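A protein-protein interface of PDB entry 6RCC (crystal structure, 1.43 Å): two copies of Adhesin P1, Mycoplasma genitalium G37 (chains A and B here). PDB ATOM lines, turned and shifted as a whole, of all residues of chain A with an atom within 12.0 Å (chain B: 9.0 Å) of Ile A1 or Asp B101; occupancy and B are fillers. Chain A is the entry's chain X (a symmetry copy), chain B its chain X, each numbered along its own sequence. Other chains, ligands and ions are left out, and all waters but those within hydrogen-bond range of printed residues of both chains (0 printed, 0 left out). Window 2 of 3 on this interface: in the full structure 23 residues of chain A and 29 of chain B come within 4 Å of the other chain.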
ATOM      1  N   ILE A   1       2.873  17.635  -8.610  1.00  0.00           N
ATOM      2  CA  ILE A   1       2.063  16.843  -7.679  1.00  0.00           C
ATOM      3  C   ILE A   1       1.464  17.725  -6.560  1.00  0.00           C
ATOM      4  O   ILE A   1       0.283  18.079  -6.647  1.00  0.00           O
ATOM      5  CB  ILE A   1       2.793  15.576  -7.132  1.00  0.00           C
ATOM      6  CG1 ILE A   1       4.351  15.731  -7.163  1.00  0.00           C
ATOM      7  CG2 ILE A   1       2.307  14.325  -7.887  1.00  0.00           C
ATOM      8  CD1 ILE A   1       5.201  14.483  -6.681  1.00  0.00           C
ATOM      9  N   SER A   2       2.268  18.123  -5.556  1.00  0.00           N
ATOM     10  CA  SER A   2       1.774  18.969  -4.460  1.00  0.00           C
ATOM     11  C   SER A   2       2.478  20.303  -4.443  1.00  0.00           C
ATOM     12  O   SER A   2       3.689  20.361  -4.637  1.00  0.00           O
ATOM     13  CB  SER A   2       1.997  18.298  -3.110  1.00  0.00           C
ATOM     14  OG  SER A   2       1.208  17.126  -3.002  1.00  0.00           O
ATOM     15  N   PHE A   3       1.730  21.355  -4.121  1.00  0.00           N
ATOM     16  CA  PHE A   3       2.247  22.708  -3.955  1.00  0.00           C
ATOM     17  C   PHE A   3       2.959  22.788  -2.606  1.00  0.00           C
ATOM     18  O   PHE A   3       2.382  22.405  -1.579  1.00  0.00           O
ATOM     19  CB  PHE A   3       1.097  23.716  -4.010  1.00  0.00           C
ATOM     20  CG  PHE A   3       1.490  25.128  -3.678  1.00  0.00           C
ATOM     21  CD1 PHE A   3       2.321  25.856  -4.529  1.00  0.00           C
ATOM     22  CD2 PHE A   3       0.960  25.767  -2.567  1.00  0.00           C
ATOM     23  CE1 PHE A   3       2.645  27.175  -4.241  1.00  0.00           C
ATOM     24  CE2 PHE A   3       1.306  27.085  -2.275  1.00  0.00           C
ATOM     25  CZ  PHE A   3       2.140  27.782  -3.128  1.00  0.00           C
ATOM     26  N   LYS A   4       4.197  23.290  -2.612  1.00  0.00           N
ATOM     27  CA  LYS A   4       4.982  23.429  -1.384  1.00  0.00           C
ATOM     28  C   LYS A   4       5.384  24.872  -1.337  1.00  0.00           C
ATOM     29  O   LYS A   4       6.286  25.294  -2.095  1.00  0.00           O
ATOM     30  CB  LYS A   4       6.213  22.517  -1.406  1.00  0.00           C
ATOM     31  CG  LYS A   4       5.850  21.037  -1.331  1.00  0.00           C
ATOM     32  CD  LYS A   4       7.069  20.159  -1.586  1.00  0.00           C
ATOM     33  CE  LYS A   4       8.041  20.147  -0.430  1.00  0.00           C
ATOM     34  NZ  LYS A   4       7.497  19.460   0.778  1.00  0.00           N
ATOM     35  N   PRO A   5       4.681  25.719  -0.575  1.00  0.00           N
ATOM     36  CA  PRO A   5       5.002  27.150  -0.602  1.00  0.00           C
ATOM     37  C   PRO A   5       6.375  27.491  -0.077  1.00  0.00           C
ATOM     38  O   PRO A   5       6.856  26.860   0.864  1.00  0.00           O
ATOM     39  CB  PRO A   5       3.941  27.791   0.278  1.00  0.00           C
ATOM     40  CG  PRO A   5       3.536  26.666   1.223  1.00  0.00           C
ATOM     41  CD  PRO A   5       3.570  25.427   0.363  1.00  0.00           C
ATOM     42  N   VAL B  59      20.041  20.965  -2.488  1.00  0.00           N
ATOM     43  CA  VAL B  59      19.544  20.811  -3.841  1.00  0.00           C
ATOM     44  C   VAL B  59      18.271  19.962  -3.818  1.00  0.00           C
ATOM     45  O   VAL B  59      17.312  20.265  -4.521  1.00  0.00           O
ATOM     46  CB  VAL B  59      20.636  20.171  -4.739  1.00  0.00           C
ATOM     47  CG1 VAL B  59      20.059  19.808  -6.103  1.00  0.00           C
ATOM     48  CG2 VAL B  59      21.820  21.128  -4.883  1.00  0.00           C
ATOM     49  N   GLU B  60      18.258  18.914  -3.001  1.00  0.00           N
ATOM     50  CA  GLU B  60      17.088  18.043  -2.921  1.00  0.00           C
ATOM     51  C   GLU B  60      15.844  18.791  -2.424  1.00  0.00           C
ATOM     52  O   GLU B  60      14.753  18.627  -2.987  1.00  0.00           O
ATOM     53  CB  GLU B  60      17.398  16.908  -1.938  1.00  0.00           C
ATOM     54  CG  GLU B  60      16.230  15.961  -1.641  1.00  0.00           C
ATOM     55  CD  GLU B  60      15.946  14.911  -2.691  1.00  0.00           C
ATOM     56  OE1 GLU B  60      16.803  14.696  -3.579  1.00  0.00           O
ATOM     57  OE2 GLU B  60      14.865  14.286  -2.613  1.00  0.00           O
ATOM     58  N   ASN B  61      16.019  19.615  -1.379  1.00  0.00           N
ATOM     59  CA  ASN B  61      14.884  20.309  -0.750  1.00  0.00           C
ATOM     60  C   ASN B  61      14.702  21.742  -1.215  1.00  0.00           C
ATOM     61  O   ASN B  61      13.735  22.398  -0.814  1.00  0.00           O
ATOM     62  CB  ASN B  61      15.001  20.253   0.774  1.00  0.00           C
ATOM     63  CG  ASN B  61      15.098  18.845   1.308  1.00  0.00           C
ATOM     64  OD1 ASN B  61      15.847  18.573   2.240  1.00  0.00           O
ATOM     65  ND2 ASN B  61      14.333  17.934   0.733  1.00  0.00           N
ATOM     66  N   GLN B  98       7.555  25.422  -4.745  1.00  0.00           N
ATOM     67  CA  GLN B  98       7.924  24.198  -5.428  1.00  0.00           C
ATOM     68  C   GLN B  98       6.702  23.353  -5.645  1.00  0.00           C
ATOM     69  O   GLN B  98       5.728  23.473  -4.902  1.00  0.00           O
ATOM     70  CB  GLN B  98       8.942  23.377  -4.620  1.00  0.00           C
ATOM     71  CG  GLN B  98      10.189  24.162  -4.216  1.00  0.00           C
ATOM     72  CD  GLN B  98      11.109  24.504  -5.370  1.00  0.00           C
ATOM     73  OE1 GLN B  98      11.276  23.740  -6.330  1.00  0.00           O
ATOM     74  NE2 GLN B  98      11.736  25.653  -5.291  1.00  0.00           N
ATOM     75  N   TRP B  99       6.759  22.495  -6.665  1.00  0.00           N
ATOM     76  CA  TRP B  99       5.696  21.539  -6.984  1.00  0.00           C
ATOM     77  C   TRP B  99       6.441  20.229  -7.036  1.00  0.00           C
ATOM     78  O   TRP B  99       7.184  19.975  -7.982  1.00  0.00           O
ATOM     79  CB  TRP B  99       4.999  21.881  -8.313  1.00  0.00           C
ATOM     80  CG  TRP B  99       4.074  23.046  -8.174  1.00  0.00           C
ATOM     81  CD1 TRP B  99       2.736  23.007  -7.900  1.00  0.00           C
ATOM     82  CD2 TRP B  99       4.431  24.431  -8.250  1.00  0.00           C
ATOM     83  NE1 TRP B  99       2.236  24.286  -7.805  1.00  0.00           N
ATOM     84  CE2 TRP B  99       3.257  25.181  -8.014  1.00  0.00           C
ATOM     85  CE3 TRP B  99       5.642  25.117  -8.458  1.00  0.00           C
ATOM     86  CZ2 TRP B  99       3.253  26.583  -8.003  1.00  0.00           C
ATOM     87  CZ3 TRP B  99       5.636  26.507  -8.443  1.00  0.00           C
ATOM     88  CH2 TRP B  99       4.447  27.224  -8.245  1.00  0.00           C
ATOM     89  N   ALA B 100       6.373  19.470  -5.948  1.00  0.00           N
ATOM     90  CA  ALA B 100       7.194  18.269  -5.813  1.00  0.00           C
ATOM     91  C   ALA B 100       6.668  17.272  -4.796  1.00  0.00           C
ATOM     92  O   ALA B 100       5.572  17.438  -4.260  1.00  0.00           O
ATOM     93  CB  ALA B 100       8.616  18.682  -5.426  1.00  0.00           C
ATOM     94  N   ASP B 101       7.493  16.237  -4.534  1.00  0.00           N
ATOM     95  CA  ASP B 101       7.306  15.110  -3.617  1.00  0.00           C
ATOM     96  C   ASP B 101       7.767  15.467  -2.206  1.00  0.00           C
ATOM     97  O   ASP B 101       7.003  15.323  -1.253  1.00  0.00           O
ATOM     98  CB  ASP B 101       8.085  13.876  -4.138  1.00  0.00           C
ATOM     99  CG  ASP B 101       9.597  14.042  -4.325  1.00  0.00           C
ATOM    100  OD1 ASP B 101      10.052  15.187  -4.564  1.00  0.00           O
ATOM    101  OD2 ASP B 101      10.318  13.024  -4.255  1.00  0.00           O
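O of Gln B98 sits at hydrogen-bond distance from N of Lys A4.
The backbone NH (N) of Ala B100 is in hydrogen-bond range of the backbone carbonyl oxygen (O) of Ser A2 (3.1 Å).
Among the printed residues, pairs that only touch across the chains: Ile A1 with Ala B100 (3.6 Å), Ile A1 with Asp B101 (3.6 Å), Ser A2 with Gln B98 (3.7 Å), Ser A2 with Trp B99 (3.3 Å), Phe A3 with Gln B98 (3.7 Å) and Phe A3 with Trp B99 (3.6 Å).
Ile A1 touches two residues of chain B.
Of chain A, only Ile A1 comes within 4 Å of Asp B101.
Of chain B, only Gln B98, Trp B99 and Ala B100 come within 4 Å of Ser A2.
Printed residues of chain A within 4 Å of Ala B100: Ile A1 and Ser A2.
Of the printed residues of chain A, Trp B99 touches Ser A2 and Phe A3.
Of the printed residues of chain B, Phe A3 touches Gln B98 and Trp B99.
Of the printed residues of chain B, Lys A4 touches Gln B98 (2.8 Å).
Printed residues of chain A within 4 Å of Gln B98: Ser A2, Phe A3 and Lys A4.
The nearest residue of chain B that does not touch Ile A1 is Trp B99 (4.7 Å).
The nearest residue of chain A that does not touch Asp B101 is Lys A4 (4.6 Å).
Hydrophobic or aromatic side chains of chain B within 4 Å of the printed part of chain A: Trp B99.
Printed residues of chain A that touch a printed residue of chain B: Ile A1, Ser A2, Phe A3 and Lys A4.
Among the printed residues, 8 pairs touch across the chains.
No position is printed for both chains.
Of the 8 pairs that touch across the chains among the printed residues, none has its exchanged pair printed and touching as well.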
